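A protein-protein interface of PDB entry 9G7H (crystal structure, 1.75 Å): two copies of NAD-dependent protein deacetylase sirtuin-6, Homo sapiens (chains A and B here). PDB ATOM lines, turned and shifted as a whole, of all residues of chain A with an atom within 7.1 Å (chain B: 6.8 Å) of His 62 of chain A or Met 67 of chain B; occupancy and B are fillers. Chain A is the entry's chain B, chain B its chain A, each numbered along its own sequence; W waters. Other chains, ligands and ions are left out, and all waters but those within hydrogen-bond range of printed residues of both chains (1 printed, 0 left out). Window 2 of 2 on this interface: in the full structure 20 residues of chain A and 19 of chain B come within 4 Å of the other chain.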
ATOM      1  N   GLY A  13      -4.922   3.591  33.111  1.00  0.00           N
ATOM      2  CA  GLY A  13      -5.083   2.988  31.801  1.00  0.00           C
ATOM      3  C   GLY A  13      -4.195   1.758  31.635  1.00  0.00           C
ATOM      4  O   GLY A  13      -3.935   1.349  30.510  1.00  0.00           O
ATOM      5  N   PRO A  56     -18.654   5.989  34.481  1.00  0.00           N
ATOM      6  CA  PRO A  56     -17.305   5.629  34.086  1.00  0.00           C
ATOM      7  C   PRO A  56     -16.530   5.532  35.392  1.00  0.00           C
ATOM      8  O   PRO A  56     -16.933   6.118  36.391  1.00  0.00           O
ATOM      9  CB  PRO A  56     -16.805   6.764  33.183  1.00  0.00           C
ATOM     10  CG  PRO A  56     -17.663   7.960  33.615  1.00  0.00           C
ATOM     11  CD  PRO A  56     -18.979   7.382  34.142  1.00  0.00           C
ATOM     12  N   ASP A  57     -15.391   4.872  35.334  1.00  0.00           N
ATOM     13  CA  ASP A  57     -14.481   4.899  36.462  1.00  0.00           C
ATOM     14  C   ASP A  57     -13.466   6.027  36.236  1.00  0.00           C
ATOM     15  O   ASP A  57     -13.721   6.931  35.465  1.00  0.00           O
ATOM     16  CB  ASP A  57     -13.937   3.504  36.678  1.00  0.00           C
ATOM     17  CG  ASP A  57     -13.072   2.892  35.591  1.00  0.00           C
ATOM     18  OD1 ASP A  57     -12.493   3.675  34.779  1.00  0.00           O
ATOM     19  OD2 ASP A  57     -12.958   1.641  35.604  1.00  0.00           O
ATOM     20  N   PHE A  58     -12.329   5.954  36.936  1.00  0.00           N
ATOM     21  CA  PHE A  58     -11.323   7.009  36.926  1.00  0.00           C
ATOM     22  C   PHE A  58     -10.086   6.588  36.137  1.00  0.00           C
ATOM     23  O   PHE A  58      -9.547   7.424  35.377  1.00  0.00           O
ATOM     24  CB  PHE A  58     -11.017   7.395  38.377  1.00  0.00           C
ATOM     25  CG  PHE A  58     -12.127   8.180  39.061  1.00  0.00           C
ATOM     26  CD1 PHE A  58     -12.304   9.544  38.817  1.00  0.00           C
ATOM     27  CD2 PHE A  58     -13.022   7.542  39.913  1.00  0.00           C
ATOM     28  CE1 PHE A  58     -13.316  10.245  39.442  1.00  0.00           C
ATOM     29  CE2 PHE A  58     -14.040   8.252  40.534  1.00  0.00           C
ATOM     30  CZ  PHE A  58     -14.190   9.598  40.287  1.00  0.00           C
ATOM     31  N   ARG A  59      -9.608   5.340  36.363  1.00  0.00           N
ATOM     32  CA  ARG A  59      -8.280   4.857  35.977  1.00  0.00           C
ATOM     33  C   ARG A  59      -8.335   3.601  35.085  1.00  0.00           C
ATOM     34  O   ARG A  59      -7.290   3.044  34.751  1.00  0.00           O
ATOM     35  CB  ARG A  59      -7.421   4.548  37.224  1.00  0.00           C
ATOM     36  CG  ARG A  59      -7.247   5.684  38.236  1.00  0.00           C
ATOM     37  CD  ARG A  59      -6.108   5.389  39.241  1.00  0.00           C
ATOM     38  NE  ARG A  59      -5.958   6.424  40.272  1.00  0.00           N
ATOM     39  CZ  ARG A  59      -6.961   6.953  41.000  1.00  0.00           C
ATOM     40  NH1 ARG A  59      -8.081   6.277  41.208  1.00  0.00           N
ATOM     41  NH2 ARG A  59      -6.814   8.123  41.604  1.00  0.00           N
ATOM     42  N   GLY A  60      -9.532   3.125  34.688  1.00  0.00           N
ATOM     43  CA  GLY A  60      -9.659   2.057  33.699  1.00  0.00           C
ATOM     44  C   GLY A  60      -9.390   2.589  32.280  1.00  0.00           C
ATOM     45  O   GLY A  60      -9.063   3.751  32.105  1.00  0.00           O
ATOM     46  N   PRO A  61      -9.516   1.764  31.218  1.00  0.00           N
ATOM     47  CA  PRO A  61      -9.179   2.187  29.854  1.00  0.00           C
ATOM     48  C   PRO A  61      -9.827   3.511  29.456  1.00  0.00           C
ATOM     49  O   PRO A  61      -9.144   4.365  28.892  1.00  0.00           O
ATOM     50  CB  PRO A  61      -9.651   1.001  28.989  1.00  0.00           C
ATOM     51  CG  PRO A  61      -9.565  -0.172  29.919  1.00  0.00           C
ATOM     52  CD  PRO A  61      -9.890   0.351  31.296  1.00  0.00           C
ATOM     53  N   HIS A  62     -11.122   3.671  29.803  1.00  0.00           N
ATOM     54  CA  HIS A  62     -11.949   4.808  29.426  1.00  0.00           C
ATOM     55  C   HIS A  62     -12.346   5.612  30.669  1.00  0.00           C
ATOM     56  O   HIS A  62     -13.361   6.300  30.697  1.00  0.00           O
ATOM     57  CB  HIS A  62     -13.159   4.313  28.625  1.00  0.00           C
ATOM     58  CG  HIS A  62     -12.780   3.796  27.275  1.00  0.00           C
ATOM     59  ND1 HIS A  62     -13.716   3.556  26.301  1.00  0.00           N
ATOM     60  CD2 HIS A  62     -11.578   3.487  26.716  1.00  0.00           C
ATOM     61  CE1 HIS A  62     -13.115   3.100  25.208  1.00  0.00           C
ATOM     62  NE2 HIS A  62     -11.810   3.042  25.440  1.00  0.00           N
ATOM     63  N   GLY A  63     -11.513   5.566  31.710  1.00  0.00           N
ATOM     64  CA  GLY A  63     -11.824   6.261  32.957  1.00  0.00           C
ATOM     65  C   GLY A  63     -11.734   7.788  32.873  1.00  0.00           C
ATOM     66  O   GLY A  63     -11.138   8.374  31.965  1.00  0.00           O
ATOM     67  N   VAL A  64     -12.278   8.465  33.891  1.00  0.00           N
ATOM     68  CA  VAL A  64     -12.217   9.913  33.947  1.00  0.00           C
ATOM     69  C   VAL A  64     -10.782  10.394  33.717  1.00  0.00           C
ATOM     70  O   VAL A  64     -10.541  11.180  32.803  1.00  0.00           O
ATOM     71  CB  VAL A  64     -12.791  10.514  35.244  1.00  0.00           C
ATOM     72  CG1 VAL A  64     -12.782  12.032  35.157  1.00  0.00           C
ATOM     73  CG2 VAL A  64     -14.213  10.036  35.515  1.00  0.00           C
ATOM     74  N   TRP A  65      -9.838   9.936  34.550  1.00  0.00           N
ATOM     75  CA  TRP A  65      -8.464  10.418  34.460  1.00  0.00           C
ATOM     76  C   TRP A  65      -7.785   9.919  33.182  1.00  0.00           C
ATOM     77  O   TRP A  65      -7.172  10.716  32.475  1.00  0.00           O
ATOM     78  CB  TRP A  65      -7.630  10.014  35.682  1.00  0.00           C
ATOM     79  CG  TRP A  65      -8.161  10.409  37.040  1.00  0.00           C
ATOM     80  CD1 TRP A  65      -7.948   9.689  38.182  1.00  0.00           C
ATOM     81  CD2 TRP A  65      -8.913  11.579  37.443  1.00  0.00           C
ATOM     82  NE1 TRP A  65      -8.532  10.306  39.258  1.00  0.00           N
ATOM     83  CE2 TRP A  65      -9.128  11.467  38.838  1.00  0.00           C
ATOM     84  CE3 TRP A  65      -9.439  12.692  36.779  1.00  0.00           C
ATOM     85  CZ2 TRP A  65      -9.830  12.426  39.565  1.00  0.00           C
ATOM     86  CZ3 TRP A  65     -10.123  13.645  37.501  1.00  0.00           C
ATOM     87  CH2 TRP A  65     -10.306  13.520  38.879  1.00  0.00           C
ATOM     88  N   THR A  66      -7.884   8.603  32.913  1.00  0.00           N
ATOM     89  CA  THR A  66      -7.298   7.970  31.731  1.00  0.00           C
ATOM     90  C   THR A  66      -7.708   8.697  30.448  1.00  0.00           C
ATOM     91  O   THR A  66      -6.910   8.791  29.511  1.00  0.00           O
ATOM     92  CB  THR A  66      -7.705   6.497  31.633  1.00  0.00           C
ATOM     93  OG1 THR A  66      -7.440   5.889  32.888  1.00  0.00           O
ATOM     94  CG2 THR A  66      -6.942   5.764  30.540  1.00  0.00           C
ATOM     95  N   MET A  67      -8.944   9.215  30.403  1.00  0.00           N
ATOM     96  CA  MET A  67      -9.452   9.873  29.210  1.00  0.00           C
ATOM     97  C   MET A  67      -8.957  11.323  29.194  1.00  0.00           C
ATOM     98  O   MET A  67      -8.550  11.800  28.152  1.00  0.00           O
ATOM     99  CB  MET A  67     -10.987   9.850  29.109  1.00  0.00           C
ATOM    100  CG  MET A  67     -11.601   8.481  28.790  1.00  0.00           C
ATOM    101  SD  MET A  67     -11.091   7.647  27.272  1.00  0.00           S
ATOM    102  CE  MET A  67     -12.365   7.870  26.027  1.00  0.00           C
ATOM    103  N   LEU A  72      -9.402  13.002  25.684  1.00  0.00           N
ATOM    104  CA  LEU A  72     -10.757  12.475  25.645  1.00  0.00           C
ATOM    105  C   LEU A  72     -11.517  12.888  26.903  1.00  0.00           C
ATOM    106  O   LEU A  72     -10.912  13.352  27.871  1.00  0.00           O
ATOM    107  CB  LEU A  72     -10.632  10.955  25.542  1.00  0.00           C
ATOM    108  CG  LEU A  72     -10.075  10.416  24.217  1.00  0.00           C
ATOM    109  CD1 LEU A  72      -9.235   9.155  24.390  1.00  0.00           C
ATOM    110  CD2 LEU A  72     -11.214  10.141  23.239  1.00  0.00           C
ATOM    111  N   ALA A  73     -12.847  12.719  26.869  1.00  0.00           N
ATOM    112  CA  ALA A  73     -13.694  12.890  28.041  1.00  0.00           C
ATOM    113  C   ALA A  73     -14.251  11.521  28.432  1.00  0.00           C
ATOM    114  O   ALA A  73     -14.465  10.684  27.568  1.00  0.00           O
ATOM    115  CB  ALA A  73     -14.830  13.864  27.763  1.00  0.00           C
ATOM    116  N   PRO A  74     -14.572  11.276  29.718  1.00  0.00           N
ATOM    117  CA  PRO A  74     -15.247  10.027  30.097  1.00  0.00           C
ATOM    118  C   PRO A  74     -16.658  10.084  29.525  1.00  0.00           C
ATOM    119  O   PRO A  74     -17.140  11.157  29.145  1.00  0.00           O
ATOM    120  CB  PRO A  74     -15.220  10.089  31.626  1.00  0.00           C
ATOM    121  CG  PRO A  74     -15.301  11.576  31.918  1.00  0.00           C
ATOM    122  CD  PRO A  74     -14.476  12.242  30.825  1.00  0.00           C
ATOM    123  N   LYS A  75     -17.329   8.926  29.485  1.00  0.00           N
ATOM    124  CA  LYS A  75     -18.681   8.869  28.971  1.00  0.00           C
ATOM    125  C   LYS A  75     -19.563   8.252  30.050  1.00  0.00           C
ATOM    126  O   LYS A  75     -19.157   7.271  30.682  1.00  0.00           O
ATOM    127  CB  LYS A  75     -18.689   8.085  27.657  1.00  0.00           C
ATOM    128  CG  LYS A  75     -20.005   7.602  27.137  1.00  0.00           C
ATOM    129  CD  LYS A  75     -20.912   8.687  26.581  1.00  0.00           C
ATOM    130  CE  LYS A  75     -22.107   8.063  25.942  1.00  0.00           C
ATOM    131  NZ  LYS A  75     -23.318   8.861  26.174  1.00  0.00           N
ATOM    132  N   GLN A 236      -7.852  -4.778  36.523  1.00  0.00           N
ATOM    133  CA  GLN A 236      -6.516  -4.237  36.358  1.00  0.00           C
ATOM    134  C   GLN A 236      -5.663  -4.551  37.578  1.00  0.00           C
ATOM    135  O   GLN A 236      -6.192  -4.908  38.631  1.00  0.00           O
ATOM    136  CB  GLN A 236      -6.575  -2.723  36.322  1.00  0.00           C
ATOM    137  CG  GLN A 236      -6.898  -2.140  34.956  1.00  0.00           C
ATOM    138  CD  GLN A 236      -6.940  -0.633  35.000  1.00  0.00           C
ATOM    139  OE1 GLN A 236      -7.066  -0.011  36.065  1.00  0.00           O
ATOM    140  NE2 GLN A 236      -6.837  -0.020  33.835  1.00  0.00           N
ATOM    141  N   CYS B  12     -20.374   8.363  12.212  1.00  0.00           N
ATOM    142  CA  CYS B  12     -19.938   7.975  13.545  1.00  0.00           C
ATOM    143  C   CYS B  12     -19.512   9.216  14.324  1.00  0.00           C
ATOM    144  O   CYS B  12     -18.878  10.139  13.766  1.00  0.00           O
ATOM    145  CB  CYS B  12     -18.826   6.943  13.466  1.00  0.00           C
ATOM    146  SG  CYS B  12     -19.279   5.474  12.515  1.00  0.00           S
ATOM    147  N   PHE B  58     -22.503   1.401  18.496  1.00  0.00           N
ATOM    148  CA  PHE B  58     -21.629   1.424  17.334  1.00  0.00           C
ATOM    149  C   PHE B  58     -21.151   2.824  16.931  1.00  0.00           C
ATOM    150  O   PHE B  58     -19.983   2.968  16.468  1.00  0.00           O
ATOM    151  CB  PHE B  58     -22.414   0.759  16.185  1.00  0.00           C
ATOM    152  CG  PHE B  58     -22.717  -0.694  16.432  1.00  0.00           C
ATOM    153  CD1 PHE B  58     -21.747  -1.665  16.149  1.00  0.00           C
ATOM    154  CD2 PHE B  58     -23.926  -1.055  17.029  1.00  0.00           C
ATOM    155  CE1 PHE B  58     -22.066  -3.001  16.418  1.00  0.00           C
ATOM    156  CE2 PHE B  58     -24.241  -2.384  17.213  1.00  0.00           C
ATOM    157  CZ  PHE B  58     -23.288  -3.331  16.902  1.00  0.00           C
ATOM    158  N   GLY B  60     -22.141   5.989  18.694  1.00  0.00           N
ATOM    159  CA  GLY B  60     -22.026   6.977  19.757  1.00  0.00           C
ATOM    160  C   GLY B  60     -20.600   7.500  19.939  1.00  0.00           C
ATOM    161  O   GLY B  60     -19.693   7.046  19.262  1.00  0.00           O
ATOM    162  N   PRO B  61     -20.321   8.442  20.881  1.00  0.00           N
ATOM    163  CA  PRO B  61     -18.959   8.969  21.018  1.00  0.00           C
ATOM    164  C   PRO B  61     -17.892   7.919  21.336  1.00  0.00           C
ATOM    165  O   PRO B  61     -16.749   8.111  20.907  1.00  0.00           O
ATOM    166  CB  PRO B  61     -19.028  10.019  22.107  1.00  0.00           C
ATOM    167  CG  PRO B  61     -20.503  10.267  22.340  1.00  0.00           C
ATOM    168  CD  PRO B  61     -21.274   9.067  21.810  1.00  0.00           C
ATOM    169  N   HIS B  62     -18.222   6.897  22.192  1.00  0.00           N
ATOM    170  CA  HIS B  62     -17.340   5.765  22.475  1.00  0.00           C
ATOM    171  C   HIS B  62     -17.783   4.481  21.775  1.00  0.00           C
ATOM    172  O   HIS B  62     -17.511   3.357  22.183  1.00  0.00           O
ATOM    173  CB  HIS B  62     -17.164   5.628  23.990  1.00  0.00           C
ATOM    174  CG  HIS B  62     -16.415   6.798  24.507  1.00  0.00           C
ATOM    175  ND1 HIS B  62     -16.054   6.866  25.832  1.00  0.00           N
ATOM    176  CD2 HIS B  62     -16.024   7.962  23.956  1.00  0.00           C
ATOM    177  CE1 HIS B  62     -15.443   8.016  26.051  1.00  0.00           C
ATOM    178  NE2 HIS B  62     -15.416   8.707  24.931  1.00  0.00           N
ATOM    179  N   GLY B  63     -18.459   4.640  20.651  1.00  0.00           N
ATOM    180  CA  GLY B  63     -18.957   3.468  19.962  1.00  0.00           C
ATOM    181  C   GLY B  63     -17.859   2.607  19.323  1.00  0.00           C
ATOM    182  O   GLY B  63     -16.726   3.069  19.064  1.00  0.00           O
ATOM    183  N   VAL B  64     -18.227   1.341  19.052  1.00  0.00           N
ATOM    184  CA  VAL B  64     -17.365   0.413  18.338  1.00  0.00           C
ATOM    185  C   VAL B  64     -16.790   1.069  17.057  1.00  0.00           C
ATOM    186  O   VAL B  64     -15.556   1.181  16.921  1.00  0.00           O
ATOM    187  CB  VAL B  64     -18.070  -0.939  18.052  1.00  0.00           C
ATOM    188  CG1 VAL B  64     -17.196  -1.874  17.242  1.00  0.00           C
ATOM    189  CG2 VAL B  64     -18.576  -1.606  19.322  1.00  0.00           C
ATOM    190  N   TRP B  65     -17.641   1.475  16.091  1.00  0.00           N
ATOM    191  CA  TRP B  65     -17.146   2.054  14.844  1.00  0.00           C
ATOM    192  C   TRP B  65     -16.491   3.430  15.042  1.00  0.00           C
ATOM    193  O   TRP B  65     -15.444   3.718  14.459  1.00  0.00           O
ATOM    194  CB  TRP B  65     -18.248   2.128  13.766  1.00  0.00           C
ATOM    195  CG  TRP B  65     -19.013   0.877  13.421  1.00  0.00           C
ATOM    196  CD1 TRP B  65     -20.303   0.893  12.972  1.00  0.00           C
ATOM    197  CD2 TRP B  65     -18.618  -0.510  13.460  1.00  0.00           C
ATOM    198  NE1 TRP B  65     -20.735  -0.372  12.708  1.00  0.00           N
ATOM    199  CE2 TRP B  65     -19.730  -1.261  13.005  1.00  0.00           C
ATOM    200  CE3 TRP B  65     -17.447  -1.193  13.818  1.00  0.00           C
ATOM    201  CZ2 TRP B  65     -19.710  -2.651  12.927  1.00  0.00           C
ATOM    202  CZ3 TRP B  65     -17.432  -2.571  13.758  1.00  0.00           C
ATOM    203  CH2 TRP B  65     -18.552  -3.291  13.328  1.00  0.00           C
ATOM    204  N   THR B  66     -17.099   4.332  15.847  1.00  0.00           N
ATOM    205  CA  THR B  66     -16.437   5.577  16.250  1.00  0.00           C
ATOM    206  C   THR B  66     -14.984   5.338  16.730  1.00  0.00           C
ATOM    207  O   THR B  66     -14.055   5.909  16.173  1.00  0.00           O
ATOM    208  CB  THR B  66     -17.287   6.267  17.307  1.00  0.00           C
ATOM    209  OG1 THR B  66     -18.599   6.434  16.728  1.00  0.00           O
ATOM    210  CG2 THR B  66     -16.776   7.666  17.637  1.00  0.00           C
ATOM    211  N   MET B  67     -14.782   4.502  17.749  1.00  0.00           N
ATOM    212  CA  MET B  67     -13.451   4.243  18.314  1.00  0.00           C
ATOM    213  C   MET B  67     -12.456   3.701  17.270  1.00  0.00           C
ATOM    214  O   MET B  67     -11.309   4.172  17.206  1.00  0.00           O
ATOM    215  CB  MET B  67     -13.515   3.303  19.519  1.00  0.00           C
ATOM    216  CG  MET B  67     -14.324   3.878  20.669  1.00  0.00           C
ATOM    217  SD  MET B  67     -13.653   5.445  21.262  1.00  0.00           S
ATOM    218  CE  MET B  67     -12.758   4.965  22.735  1.00  0.00           C
ATOM    219  N   GLU B  68     -12.881   2.712  16.479  1.00  0.00           N
ATOM    220  CA  GLU B  68     -12.139   2.165  15.357  1.00  0.00           C
ATOM    221  C   GLU B  68     -11.627   3.290  14.445  1.00  0.00           C
ATOM    222  O   GLU B  68     -10.460   3.281  14.028  1.00  0.00           O
ATOM    223  CB  GLU B  68     -13.100   1.206  14.661  1.00  0.00           C
ATOM    224  CG  GLU B  68     -12.527   0.564  13.404  1.00  0.00           C
ATOM    225  CD  GLU B  68     -13.543  -0.188  12.562  1.00  0.00           C
ATOM    226  OE1 GLU B  68     -14.036   0.373  11.554  1.00  0.00           O
ATOM    227  OE2 GLU B  68     -13.799  -1.363  12.888  1.00  0.00           O
ATOM    228  N   GLU B  69     -12.510   4.250  14.099  1.00  0.00           N
ATOM    229  CA  GLU B  69     -12.150   5.433  13.316  1.00  0.00           C
ATOM    230  C   GLU B  69     -11.018   6.257  13.948  1.00  0.00           C
ATOM    231  O   GLU B  69     -10.244   6.915  13.252  1.00  0.00           O
ATOM    232  CB  GLU B  69     -13.328   6.409  13.165  1.00  0.00           C
ATOM    233  CG  GLU B  69     -14.338   5.996  12.103  1.00  0.00           C
ATOM    234  CD  GLU B  69     -15.357   7.065  11.700  1.00  0.00           C
ATOM    235  OE1 GLU B  69     -15.448   8.135  12.317  1.00  0.00           O
ATOM    236  OE2 GLU B  69     -16.013   6.828  10.673  1.00  0.00           O
ATOM    237  N   ARG B  70     -10.981   6.357  15.270  1.00  0.00           N
ATOM    238  CA  ARG B  70      -9.937   7.126  15.937  1.00  0.00           C
ATOM    239  C   ARG B  70      -8.726   6.260  16.272  1.00  0.00           C
ATOM    240  O   ARG B  70      -7.831   6.743  16.957  1.00  0.00           O
ATOM    241  CB  ARG B  70     -10.438   7.698  17.267  1.00  0.00           C
ATOM    242  CG  ARG B  70     -11.243   8.983  17.176  1.00  0.00           C
ATOM    243  CD  ARG B  70     -12.473   8.800  16.314  1.00  0.00           C
ATOM    244  NE  ARG B  70     -13.475   9.840  16.568  1.00  0.00           N
ATOM    245  CZ  ARG B  70     -14.601  10.019  15.884  1.00  0.00           C
ATOM    246  NH1 ARG B  70     -14.890   9.225  14.860  1.00  0.00           N
ATOM    247  NH2 ARG B  70     -15.440  10.982  16.253  1.00  0.00           N
ATOM    248  N   GLY B  71      -8.701   5.001  15.817  1.00  0.00           N
ATOM    249  CA  GLY B  71      -7.652   4.054  16.150  1.00  0.00           C
ATOM    250  C   GLY B  71      -7.722   3.545  17.596  1.00  0.00           C
ATOM    251  O   GLY B  71      -6.727   3.102  18.151  1.00  0.00           O
ATOM    252  N   LEU B  72      -8.885   3.617  18.239  1.00  0.00           N
ATOM    253  CA  LEU B  72      -8.948   3.181  19.627  1.00  0.00           C
ATOM    254  C   LEU B  72      -9.921   2.020  19.755  1.00  0.00           C
ATOM    255  O   LEU B  72     -10.503   1.556  18.783  1.00  0.00           O
ATOM    256  CB  LEU B  72      -9.375   4.329  20.531  1.00  0.00           C
ATOM    257  CG  LEU B  72      -8.469   5.557  20.621  1.00  0.00           C
ATOM    258  CD1 LEU B  72      -9.371   6.771  20.770  1.00  0.00           C
ATOM    259  CD2 LEU B  72      -7.510   5.370  21.799  1.00  0.00           C
ATOM    260  N   ALA B  73     -10.115   1.561  20.988  1.00  0.00           N
ATOM    261  CA  ALA B  73     -10.882   0.349  21.218  1.00  0.00           C
ATOM    262  C   ALA B  73     -12.170   0.686  21.954  1.00  0.00           C
ATOM    263  O   ALA B  73     -12.173   1.580  22.806  1.00  0.00           O
ATOM    264  CB  ALA B  73     -10.051  -0.638  22.008  1.00  0.00           C
ATOM    265  N   PRO B  74     -13.286  -0.032  21.695  1.00  0.00           N
ATOM    266  CA  PRO B  74     -14.478   0.097  22.538  1.00  0.00           C
ATOM    267  C   PRO B  74     -14.176  -0.570  23.873  1.00  0.00           C
ATOM    268  O   PRO B  74     -13.184  -1.285  23.958  1.00  0.00           O
ATOM    269  CB  PRO B  74     -15.549  -0.636  21.726  1.00  0.00           C
ATOM    270  CG  PRO B  74     -14.775  -1.725  21.043  1.00  0.00           C
ATOM    271  CD  PRO B  74     -13.479  -1.033  20.632  1.00  0.00           C
ATOM    272  N   LYS B  75     -14.959  -0.207  24.898  1.00  0.00           N
ATOM    273  CA  LYS B  75     -14.864  -0.786  26.226  1.00  0.00           C
ATOM    274  C   LYS B  75     -16.181  -1.484  26.555  1.00  0.00           C
ATOM    275  O   LYS B  75     -17.283  -1.005  26.263  1.00  0.00           O
ATOM    276  CB  LYS B  75     -14.524   0.322  27.221  1.00  0.00           C
ATOM    277  CG  LYS B  75     -14.506  -0.020  28.689  1.00  0.00           C
ATOM    278  CD  LYS B  75     -13.615  -1.178  29.108  1.00  0.00           C
ATOM    279  CE  LYS B  75     -13.717  -1.339  30.605  1.00  0.00           C
ATOM    280  NZ  LYS B  75     -13.476  -2.715  31.026  1.00  0.00           N
ATOM    281  N   PHE B  76     -16.023  -2.702  27.074  1.00  0.00           N
ATOM    282  CA  PHE B  76     -17.127  -3.461  27.636  1.00  0.00           C
ATOM    283  C   PHE B  76     -16.955  -3.456  29.149  1.00  0.00           C
ATOM    284  O   PHE B  76     -15.852  -3.694  29.641  1.00  0.00           O
ATOM    285  CB  PHE B  76     -17.250  -4.922  27.231  1.00  0.00           C
ATOM    286  CG  PHE B  76     -17.905  -5.205  25.876  1.00  0.00           C
ATOM    287  CD1 PHE B  76     -17.268  -4.862  24.699  1.00  0.00           C
ATOM    288  CD2 PHE B  76     -19.141  -5.826  25.813  1.00  0.00           C
ATOM    289  CE1 PHE B  76     -17.854  -5.158  23.473  1.00  0.00           C
ATOM    290  CE2 PHE B  76     -19.713  -6.125  24.589  1.00  0.00           C
ATOM    291  CZ  PHE B  76     -19.059  -5.790  23.426  1.00  0.00           C
HETATM  292  O   HOH W   1      -9.256   2.784  23.829  1.00  0.00           O
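Pro 56 of chain A touches none of the printed residues of chain B.
Printed residues of chain B within 4 Å of His 62 of chain A: Met 67, Ala 73 and Lys 75.
Of the printed residues of chain B, Ala 73 of chain A touches His 62 (3.2 Å).
Printed residues of chain B within 4 Å of Lys 75 of chain A: His 62 (3.4 Å).
Of the printed residues of chain A, His 62 of chain B touches Met 67, Ala 73 and Lys 75.
Val 64 of chain B touches none of the printed residues of chain A.
Of the printed residues of chain A, Met 67 of chain B touches His 62 (3.1 Å).
Of the printed residues of chain A, Ala 73 of chain B touches His 62.
Of the printed residues of chain A, Lys 75 of chain B touches His 62.
The nearest printed residue of chain A that does not touch Lys 75 of chain B is Pro 61 of chain A (4.2 Å).
NE2 of His 62 of chain B lies close to O of Ala 73 of chain A, at 3.4 Å.
The backbone carbonyl oxygen (O) of Ala 73 of chain B lies close to a ring nitrogen (NE2) of His 62 of chain A, 3.0 Å away.
N of Leu 72 of chain B lies within hydrogen-bond range of O of Met 67 of chain B (2.7 Å).
O of Met 67 of chain A sits at hydrogen-bond distance from N of Leu 72 of chain A.
His 62 of chain A touches Met 67 of chain B, and with the chains exchanged Met 67 of chain A touches His 62 of chain B.
His 62 of chain A touches Ala 73 of chain B, and with the chains exchanged Ala 73 of chain A touches His 62 of chain B.
His 62 of chain A touches Lys 75 of chain B, and with the chains exchanged Lys 75 of chain A touches His 62 of chain B.
Water W1 bridges NE2 of His 62 of chain A (3.0 Å) and N of Ala 73 of chain B (3.2 Å).
Among the printed residues, pairs that only touch across the chains: His 62 of chain A with Met 67 of chain B (3.1 Å), His 62 of chain A with Lys 75 of chain B (3.5 Å), Met 67 of chain A with His 62 of chain B (3.1 Å) and Lys 75 of chain A with His 62 of chain B (3.4 Å).
Hydrophobic or aromatic side chains of chain B that line the printed part of chain A: His 62 and Met 67.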
